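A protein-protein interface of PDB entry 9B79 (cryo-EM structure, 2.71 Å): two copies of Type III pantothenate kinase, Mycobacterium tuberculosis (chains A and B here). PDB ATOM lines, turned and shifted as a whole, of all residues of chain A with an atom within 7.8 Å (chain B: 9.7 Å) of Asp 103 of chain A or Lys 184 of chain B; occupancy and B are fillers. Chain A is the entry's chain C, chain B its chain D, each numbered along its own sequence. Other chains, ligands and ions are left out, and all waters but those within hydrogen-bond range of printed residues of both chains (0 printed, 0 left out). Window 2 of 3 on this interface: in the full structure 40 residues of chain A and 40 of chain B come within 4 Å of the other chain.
N of Val 140 of chain A sits at hydrogen-bond distance from O of Gly 149 of chain A (2.9 Å).
The side-chain amide oxygen of Asn 185 of chain B lies within hydrogen-bond range of the backbone NH of Glu 188 of chain B, 2.8 Å away.
The side-chain amide oxygen (OD1) of Asn 185 of chain B sits close to the backbone NH (N) of Val 187 of chain B.
The backbone carbonyl oxygen of Asn 185 of chain B lies close to the side-chain sulfur of Cys 189 of chain B (3.6 Å).
N of Leu 148 of chain A lies within hydrogen-bond range of O of Val 140 of chain A, at 3.3 Å.
Lys 184 of chain B touches Val 102 of chain A.
ND2 of Asn 104 of chain A touches CB of Asn 185 of chain B, at 3.3 Å.
Gly 149 of chain A touches Val 182 of chain B (C to CG1, 3.6 Å).
CG1 of Val 182 of chain B touches N of Gly 150 of chain A, at 3.6 Å.
Val 213 of chain A touches Val 182 of chain B (CG2 to CG2, 3.7 Å).
The side-chain sulfur (SG) of Cys 189 of chain B is in hydrogen-bond range of the backbone carbonyl oxygen (O) of Gly 150 of chain A (3.6 Å).
O of Leu 148 of chain A sits at hydrogen-bond distance from NZ of Lys 184 of chain B, at 3.4 Å.
The backbone carbonyl oxygen (O) of Val 181 of chain B lies close to the backbone carbonyl oxygen (O) of Gly 150 of chain A.
N of Asp 103 of chain A lies close to O of Lys 184 of chain B.
The backbone NH (N) of Gly 183 of chain B lies within hydrogen-bond range of the backbone carbonyl oxygen (O) of Gly 150 of chain A (3.2 Å).
Of chain B, only Lys 184 (3.4 Å) comes within 4 Å of Asp 103 of chain A.
Lys 184 of chain B touches three residues of chain A.
Val 102 of chain A touches one residue of chain B.
Of chain B, only Asn 185 (3.3 Å) comes within 4 Å of Asn 104 of chain A.
Of chain A, only Gly 150 (3.2 Å) comes within 4 Å of Gly 183 of chain B.
Of the printed residues of chain A, Cys 189 of chain B touches Gly 150.
Of the printed residues of chain A, Asn 185 of chain B touches Asn 104 (3.3 Å).
Printed residues of chain A within 4 Å of Val 182 of chain B: Gly 149, Gly 150 and Val 213.
The nearest residue of chain A that does not touch Lys 184 of chain B is Asn 104 of chain A (4.05 Å).
The nearest printed residue of chain B that does not touch Val 213 of chain A is Val 181 of chain B (6.3 Å).
No position is printed for both chains.
Of the 10 pairs that touch across the chains among the printed residues, none has its exchanged pair printed and touching as well.
Printed residues of chain B that touch a printed residue of chain A: Val 181, Val 182, Gly 183, Lys 184, Asn 185 and Cys 189.
Of the 15 printed residues of chain A, 7 touch a printed residue of chain B.
Among the printed residues, no Asp or Glu carboxylate lies within 4 Å of a Lys or Arg side-chain nitrogen of the other chain.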
ATOM      1  N   LEU A 100     -11.317  -3.033  18.516  1.00  0.00           N
ATOM      2  CA  LEU A 100     -11.389  -3.714  17.223  1.00  0.00           C
ATOM      3  C   LEU A 100     -11.513  -5.220  17.446  1.00  0.00           C
ATOM      4  O   LEU A 100     -10.550  -5.976  17.325  1.00  0.00           O
ATOM      5  CB  LEU A 100     -10.169  -3.372  16.371  1.00  0.00           C
ATOM      6  CG  LEU A 100     -10.320  -2.286  15.302  1.00  0.00           C
ATOM      7  CD1 LEU A 100     -10.826  -0.985  15.901  1.00  0.00           C
ATOM      8  CD2 LEU A 100      -9.001  -2.067  14.580  1.00  0.00           C
ATOM      9  N   LEU A 101     -12.730  -5.657  17.772  1.00  0.00           N
ATOM     10  CA  LEU A 101     -13.007  -7.080  17.978  1.00  0.00           C
ATOM     11  C   LEU A 101     -13.078  -7.749  16.609  1.00  0.00           C
ATOM     12  O   LEU A 101     -14.146  -8.063  16.079  1.00  0.00           O
ATOM     13  CB  LEU A 101     -14.287  -7.283  18.781  1.00  0.00           C
ATOM     14  CG  LEU A 101     -14.179  -7.240  20.310  1.00  0.00           C
ATOM     15  CD1 LEU A 101     -13.788  -5.867  20.827  1.00  0.00           C
ATOM     16  CD2 LEU A 101     -15.485  -7.696  20.941  1.00  0.00           C
ATOM     17  N   VAL A 102     -11.895  -7.981  16.035  1.00  0.00           N
ATOM     18  CA  VAL A 102     -11.733  -8.576  14.715  1.00  0.00           C
ATOM     19  C   VAL A 102     -10.489  -9.455  14.796  1.00  0.00           C
ATOM     20  O   VAL A 102      -9.649  -9.291  15.684  1.00  0.00           O
ATOM     21  CB  VAL A 102     -11.591  -7.477  13.610  1.00  0.00           C
ATOM     22  CG1 VAL A 102     -11.319  -8.042  12.221  1.00  0.00           C
ATOM     23  CG2 VAL A 102     -12.817  -6.582  13.548  1.00  0.00           C
ATOM     24  N   ASP A 103     -10.381 -10.412  13.868  1.00  0.00           N
ATOM     25  CA  ASP A 103      -9.271 -11.358  13.905  1.00  0.00           C
ATOM     26  C   ASP A 103      -7.944 -10.650  13.669  1.00  0.00           C
ATOM     27  O   ASP A 103      -6.930 -10.993  14.287  1.00  0.00           O
ATOM     28  CB  ASP A 103      -9.487 -12.457  12.865  1.00  0.00           C
ATOM     29  CG  ASP A 103     -10.664 -13.351  13.199  1.00  0.00           C
ATOM     30  OD1 ASP A 103     -11.283 -13.147  14.265  1.00  0.00           O
ATOM     31  OD2 ASP A 103     -10.973 -14.254  12.395  1.00  0.00           O
ATOM     32  N   ASN A 104      -7.934  -9.661  12.779  1.00  0.00           N
ATOM     33  CA  ASN A 104      -6.730  -8.907  12.426  1.00  0.00           C
ATOM     34  C   ASN A 104      -6.978  -7.403  12.555  1.00  0.00           C
ATOM     35  O   ASN A 104      -7.228  -6.695  11.574  1.00  0.00           O
ATOM     36  CB  ASN A 104      -6.183  -9.398  11.072  1.00  0.00           C
ATOM     37  CG  ASN A 104      -7.143  -9.202   9.875  1.00  0.00           C
ATOM     38  OD1 ASN A 104      -7.917  -8.258   9.773  1.00  0.00           O
ATOM     39  ND2 ASN A 104      -7.062 -10.144   8.943  1.00  0.00           N
ATOM     40  N   PRO A 105      -6.854  -6.867  13.774  1.00  0.00           N
ATOM     41  CA  PRO A 105      -7.062  -5.422  13.963  1.00  0.00           C
ATOM     42  C   PRO A 105      -6.027  -4.559  13.265  1.00  0.00           C
ATOM     43  O   PRO A 105      -6.281  -3.366  13.062  1.00  0.00           O
ATOM     44  CB  PRO A 105      -6.991  -5.249  15.489  1.00  0.00           C
ATOM     45  CG  PRO A 105      -7.158  -6.633  16.054  1.00  0.00           C
ATOM     46  CD  PRO A 105      -6.557  -7.552  15.043  1.00  0.00           C
ATOM     47  N   LYS A 106      -4.870  -5.116  12.903  1.00  0.00           N
ATOM     48  CA  LYS A 106      -3.840  -4.325  12.239  1.00  0.00           C
ATOM     49  C   LYS A 106      -4.284  -3.883  10.851  1.00  0.00           C
ATOM     50  O   LYS A 106      -3.993  -2.759  10.429  1.00  0.00           O
ATOM     51  CB  LYS A 106      -2.534  -5.116  12.160  1.00  0.00           C
ATOM     52  CG  LYS A 106      -1.883  -5.376  13.507  1.00  0.00           C
ATOM     53  CD  LYS A 106      -0.606  -6.184  13.356  1.00  0.00           C
ATOM     54  CE  LYS A 106       0.061  -6.423  14.701  1.00  0.00           C
ATOM     55  NZ  LYS A 106       1.300  -7.235  14.565  1.00  0.00           N
ATOM     56  N   GLU A 107      -4.984  -4.752  10.127  1.00  0.00           N
ATOM     57  CA  GLU A 107      -5.288  -4.518   8.721  1.00  0.00           C
ATOM     58  C   GLU A 107      -6.611  -3.797   8.501  1.00  0.00           C
ATOM     59  O   GLU A 107      -7.001  -3.594   7.347  1.00  0.00           O
ATOM     60  CB  GLU A 107      -5.300  -5.848   7.960  1.00  0.00           C
ATOM     61  CG  GLU A 107      -4.056  -6.703   8.163  1.00  0.00           C
ATOM     62  CD  GLU A 107      -2.806  -6.084   7.567  1.00  0.00           C
ATOM     63  OE1 GLU A 107      -2.178  -5.235   8.237  1.00  0.00           O
ATOM     64  OE2 GLU A 107      -2.450  -6.446   6.426  1.00  0.00           O
ATOM     65  N   VAL A 108      -7.312  -3.412   9.567  1.00  0.00           N
ATOM     66  CA  VAL A 108      -8.574  -2.697   9.409  1.00  0.00           C
ATOM     67  C   VAL A 108      -8.287  -1.290   8.906  1.00  0.00           C
ATOM     68  O   VAL A 108      -7.427  -0.585   9.449  1.00  0.00           O
ATOM     69  CB  VAL A 108      -9.348  -2.674  10.735  1.00  0.00           C
ATOM     70  CG1 VAL A 108     -10.595  -1.814  10.609  1.00  0.00           C
ATOM     71  CG2 VAL A 108      -9.715  -4.087  11.155  1.00  0.00           C
ATOM     72  N   VAL A 140     -20.319  -2.377  11.042  1.00  0.00           N
ATOM     73  CA  VAL A 140     -21.305  -2.521  12.104  1.00  0.00           C
ATOM     74  C   VAL A 140     -20.623  -2.263  13.441  1.00  0.00           C
ATOM     75  O   VAL A 140     -19.502  -2.724  13.681  1.00  0.00           O
ATOM     76  CB  VAL A 140     -22.006  -3.897  12.077  1.00  0.00           C
ATOM     77  CG1 VAL A 140     -22.758  -4.054  10.779  1.00  0.00           C
ATOM     78  CG2 VAL A 140     -21.023  -5.037  12.257  1.00  0.00           C
ATOM     79  N   PHE A 147     -16.235  -2.748  17.437  1.00  0.00           N
ATOM     80  CA  PHE A 147     -16.251  -2.824  15.981  1.00  0.00           C
ATOM     81  C   PHE A 147     -16.206  -4.289  15.565  1.00  0.00           C
ATOM     82  O   PHE A 147     -15.179  -4.956  15.720  1.00  0.00           O
ATOM     83  CB  PHE A 147     -15.082  -2.048  15.380  1.00  0.00           C
ATOM     84  CG  PHE A 147     -14.800  -2.397  13.947  1.00  0.00           C
ATOM     85  CD1 PHE A 147     -15.718  -2.096  12.955  1.00  0.00           C
ATOM     86  CD2 PHE A 147     -13.615  -3.016  13.590  1.00  0.00           C
ATOM     87  CE1 PHE A 147     -15.464  -2.414  11.637  1.00  0.00           C
ATOM     88  CE2 PHE A 147     -13.356  -3.334  12.271  1.00  0.00           C
ATOM     89  CZ  PHE A 147     -14.282  -3.032  11.295  1.00  0.00           C
ATOM     90  N   LEU A 148     -17.322  -4.787  15.032  1.00  0.00           N
ATOM     91  CA  LEU A 148     -17.414  -6.196  14.669  1.00  0.00           C
ATOM     92  C   LEU A 148     -16.791  -6.457  13.303  1.00  0.00           C
ATOM     93  O   LEU A 148     -15.942  -7.344  13.159  1.00  0.00           O
ATOM     94  CB  LEU A 148     -18.872  -6.652  14.692  1.00  0.00           C
ATOM     95  CG  LEU A 148     -19.637  -6.376  15.988  1.00  0.00           C
ATOM     96  CD1 LEU A 148     -21.060  -6.892  15.883  1.00  0.00           C
ATOM     97  CD2 LEU A 148     -18.919  -7.000  17.174  1.00  0.00           C
ATOM     98  N   GLY A 149     -17.206  -5.711  12.300  1.00  0.00           N
ATOM     99  CA  GLY A 149     -16.745  -5.918  10.943  1.00  0.00           C
ATOM    100  C   GLY A 149     -17.825  -5.506   9.959  1.00  0.00           C
ATOM    101  O   GLY A 149     -18.634  -4.625  10.243  1.00  0.00           O
ATOM    102  N   GLY A 150     -17.819  -6.159   8.803  1.00  0.00           N
ATOM    103  CA  GLY A 150     -18.791  -5.838   7.781  1.00  0.00           C
ATOM    104  C   GLY A 150     -18.461  -6.429   6.429  1.00  0.00           C
ATOM    105  O   GLY A 150     -18.221  -7.633   6.311  1.00  0.00           O
ATOM    106  N   VAL A 213     -27.154 -11.364  12.561  1.00  0.00           N
ATOM    107  CA  VAL A 213     -26.293 -10.971  13.672  1.00  0.00           C
ATOM    108  C   VAL A 213     -27.162 -10.628  14.874  1.00  0.00           C
ATOM    109  O   VAL A 213     -28.185  -9.947  14.741  1.00  0.00           O
ATOM    110  CB  VAL A 213     -25.376  -9.785  13.303  1.00  0.00           C
ATOM    111  CG1 VAL A 213     -24.421  -9.474  14.441  1.00  0.00           C
ATOM    112  CG2 VAL A 213     -24.593 -10.090  12.037  1.00  0.00           C
ATOM    113  N   PRO B 178     -18.414 -16.825   1.897  1.00  0.00           N
ATOM    114  CA  PRO B 178     -17.755 -16.849   3.207  1.00  0.00           C
ATOM    115  C   PRO B 178     -18.631 -17.469   4.284  1.00  0.00           C
ATOM    116  O   PRO B 178     -19.725 -17.963   3.992  1.00  0.00           O
ATOM    117  CB  PRO B 178     -17.498 -15.366   3.482  1.00  0.00           C
ATOM    118  CG  PRO B 178     -18.677 -14.707   2.864  1.00  0.00           C
ATOM    119  CD  PRO B 178     -19.038 -15.517   1.631  1.00  0.00           C
ATOM    120  N   ARG B 179     -18.155 -17.453   5.532  1.00  0.00           N
ATOM    121  CA  ARG B 179     -18.933 -18.012   6.633  1.00  0.00           C
ATOM    122  C   ARG B 179     -20.201 -17.204   6.878  1.00  0.00           C
ATOM    123  O   ARG B 179     -21.303 -17.761   6.943  1.00  0.00           O
ATOM    124  CB  ARG B 179     -18.086 -18.059   7.904  1.00  0.00           C
ATOM    125  CG  ARG B 179     -16.836 -18.909   7.807  1.00  0.00           C
ATOM    126  CD  ARG B 179     -15.693 -18.250   8.560  1.00  0.00           C
ATOM    127  NE  ARG B 179     -16.150 -17.649   9.807  1.00  0.00           N
ATOM    128  CZ  ARG B 179     -15.403 -16.875  10.583  1.00  0.00           C
ATOM    129  NH1 ARG B 179     -14.149 -16.586  10.273  1.00  0.00           N
ATOM    130  NH2 ARG B 179     -15.928 -16.374  11.699  1.00  0.00           N
ATOM    131  N   SER B 180     -20.066 -15.887   7.013  1.00  0.00           N
ATOM    132  CA  SER B 180     -21.203 -15.020   7.283  1.00  0.00           C
ATOM    133  C   SER B 180     -20.987 -13.693   6.570  1.00  0.00           C
ATOM    134  O   SER B 180     -19.936 -13.447   5.974  1.00  0.00           O
ATOM    135  CB  SER B 180     -21.403 -14.805   8.786  1.00  0.00           C
ATOM    136  OG  SER B 180     -21.803 -16.007   9.422  1.00  0.00           O
ATOM    137  N   VAL B 181     -22.009 -12.837   6.635  1.00  0.00           N
ATOM    138  CA  VAL B 181     -21.937 -11.543   5.963  1.00  0.00           C
ATOM    139  C   VAL B 181     -20.914 -10.643   6.645  1.00  0.00           C
ATOM    140  O   VAL B 181     -20.131  -9.954   5.981  1.00  0.00           O
ATOM    141  CB  VAL B 181     -23.331 -10.894   5.915  1.00  0.00           C
ATOM    142  CG1 VAL B 181     -23.250  -9.509   5.302  1.00  0.00           C
ATOM    143  CG2 VAL B 181     -24.295 -11.771   5.136  1.00  0.00           C
ATOM    144  N   VAL B 182     -20.893 -10.641   7.977  1.00  0.00           N
ATOM    145  CA  VAL B 182     -19.916  -9.863   8.731  1.00  0.00           C
ATOM    146  C   VAL B 182     -18.615 -10.650   8.817  1.00  0.00           C
ATOM    147  O   VAL B 182     -18.443 -11.494   9.704  1.00  0.00           O
ATOM    148  CB  VAL B 182     -20.445  -9.506  10.132  1.00  0.00           C
ATOM    149  CG1 VAL B 182     -19.448  -8.632  10.870  1.00  0.00           C
ATOM    150  CG2 VAL B 182     -21.784  -8.806  10.024  1.00  0.00           C
ATOM    151  N   GLY B 183     -17.697 -10.386   7.894  1.00  0.00           N
ATOM    152  CA  GLY B 183     -16.420 -11.065   7.898  1.00  0.00           C
ATOM    153  C   GLY B 183     -15.522 -10.617   9.035  1.00  0.00           C
ATOM    154  O   GLY B 183     -15.802  -9.667   9.768  1.00  0.00           O
ATOM    155  N   LYS B 184     -14.406 -11.333   9.181  1.00  0.00           N
ATOM    156  CA  LYS B 184     -13.435 -11.055  10.232  1.00  0.00           C
ATOM    157  C   LYS B 184     -12.029 -10.845   9.683  1.00  0.00           C
ATOM    158  O   LYS B 184     -11.081 -10.737  10.468  1.00  0.00           O
ATOM    159  CB  LYS B 184     -13.421 -12.181  11.272  1.00  0.00           C
ATOM    160  CG  LYS B 184     -14.767 -12.446  11.924  1.00  0.00           C
ATOM    161  CD  LYS B 184     -15.236 -11.255  12.742  1.00  0.00           C
ATOM    162  CE  LYS B 184     -16.633 -11.488  13.292  1.00  0.00           C
ATOM    163  NZ  LYS B 184     -17.094 -10.361  14.146  1.00  0.00           N
ATOM    164  N   ASN B 185     -11.867 -10.802   8.364  1.00  0.00           N
ATOM    165  CA  ASN B 185     -10.578 -10.509   7.756  1.00  0.00           C
ATOM    166  C   ASN B 185     -10.820  -9.927   6.373  1.00  0.00           C
ATOM    167  O   ASN B 185     -11.939  -9.951   5.854  1.00  0.00           O
ATOM    168  CB  ASN B 185      -9.693 -11.758   7.681  1.00  0.00           C
ATOM    169  CG  ASN B 185     -10.365 -12.907   6.958  1.00  0.00           C
ATOM    170  OD1 ASN B 185     -10.222 -13.061   5.745  1.00  0.00           O
ATOM    171  ND2 ASN B 185     -11.098 -13.726   7.703  1.00  0.00           N
ATOM    172  N   THR B 186      -9.751  -9.383   5.785  1.00  0.00           N
ATOM    173  CA  THR B 186      -9.882  -8.668   4.519  1.00  0.00           C
ATOM    174  C   THR B 186     -10.384  -9.588   3.415  1.00  0.00           C
ATOM    175  O   THR B 186     -11.247  -9.203   2.620  1.00  0.00           O
ATOM    176  CB  THR B 186      -8.544  -8.039   4.130  1.00  0.00           C
ATOM    177  OG1 THR B 186      -8.058  -7.240   5.216  1.00  0.00           O
ATOM    178  CG2 THR B 186      -8.705  -7.161   2.900  1.00  0.00           C
ATOM    179  N   VAL B 187      -9.853 -10.812   3.354  1.00  0.00           N
ATOM    180  CA  VAL B 187     -10.309 -11.782   2.361  1.00  0.00           C
ATOM    181  C   VAL B 187     -11.782 -12.105   2.577  1.00  0.00           C
ATOM    182  O   VAL B 187     -12.580 -12.130   1.631  1.00  0.00           O
ATOM    183  CB  VAL B 187      -9.442 -13.051   2.419  1.00  0.00           C
ATOM    184  CG1 VAL B 187      -9.904 -14.064   1.389  1.00  0.00           C
ATOM    185  CG2 VAL B 187      -7.986 -12.696   2.208  1.00  0.00           C
ATOM    186  N   GLU B 188     -12.163 -12.340   3.834  1.00  0.00           N
ATOM    187  CA  GLU B 188     -13.545 -12.682   4.140  1.00  0.00           C
ATOM    188  C   GLU B 188     -14.473 -11.498   3.905  1.00  0.00           C
ATOM    189  O   GLU B 188     -15.590 -11.675   3.410  1.00  0.00           O
ATOM    190  CB  GLU B 188     -13.659 -13.178   5.581  1.00  0.00           C
ATOM    191  CG  GLU B 188     -14.996 -13.821   5.913  1.00  0.00           C
ATOM    192  CD  GLU B 188     -15.034 -14.393   7.318  1.00  0.00           C
ATOM    193  OE1 GLU B 188     -13.961 -14.758   7.843  1.00  0.00           O
ATOM    194  OE2 GLU B 188     -16.137 -14.478   7.898  1.00  0.00           O
ATOM    195  N   CYS B 189     -14.027 -10.284   4.244  1.00  0.00           N
ATOM    196  CA  CYS B 189     -14.840  -9.101   3.978  1.00  0.00           C
ATOM    197  C   CYS B 189     -15.046  -8.890   2.484  1.00  0.00           C
ATOM    198  O   CYS B 189     -16.160  -8.591   2.042  1.00  0.00           O
ATOM    199  CB  CYS B 189     -14.197  -7.863   4.606  1.00  0.00           C
ATOM    200  SG  CYS B 189     -14.612  -7.580   6.342  1.00  0.00           S
ATOM    201  N   MET B 190     -13.983  -9.040   1.688  1.00  0.00           N
ATOM    202  CA  MET B 190     -14.110  -8.881   0.242  1.00  0.00           C
ATOM    203  C   MET B 190     -15.017  -9.944  -0.365  1.00  0.00           C
ATOM    204  O   MET B 190     -15.843  -9.641  -1.235  1.00  0.00           O
ATOM    205  CB  MET B 190     -12.731  -8.916  -0.414  1.00  0.00           C
ATOM    206  CG  MET B 190     -11.885  -7.685  -0.150  1.00  0.00           C
ATOM    207  SD  MET B 190     -10.272  -7.785  -0.940  1.00  0.00           S
ATOM    208  CE  MET B 190     -10.753  -8.156  -2.623  1.00  0.00           C
ATOM    209  N   GLN B 191     -14.872 -11.201   0.070  1.00  0.00           N
ATOM    210  CA  GLN B 191     -15.737 -12.258  -0.446  1.00  0.00           C
ATOM    211  C   GLN B 191     -17.187 -12.041  -0.036  1.00  0.00           C
ATOM    212  O   GLN B 191     -18.098 -12.229  -0.850  1.00  0.00           O
ATOM    213  CB  GLN B 191     -15.246 -13.621   0.035  1.00  0.00           C
ATOM    214  CG  GLN B 191     -14.009 -14.121  -0.680  1.00  0.00           C
ATOM    215  CD  GLN B 191     -13.578 -15.487  -0.200  1.00  0.00           C
ATOM    216  OE1 GLN B 191     -14.001 -15.947   0.860  1.00  0.00           O
ATOM    217  NE2 GLN B 191     -12.734 -16.150  -0.980  1.00  0.00           N
ATOM    218  N   ALA B 192     -17.419 -11.629   1.214  1.00  0.00           N
ATOM    219  CA  ALA B 192     -18.773 -11.338   1.665  1.00  0.00           C
ATOM    220  C   ALA B 192     -19.382 -10.204   0.863  1.00  0.00           C
ATOM    221  O   ALA B 192     -20.527 -10.304   0.409  1.00  0.00           O
ATOM    222  CB  ALA B 192     -18.770 -10.997   3.154  1.00  0.00           C
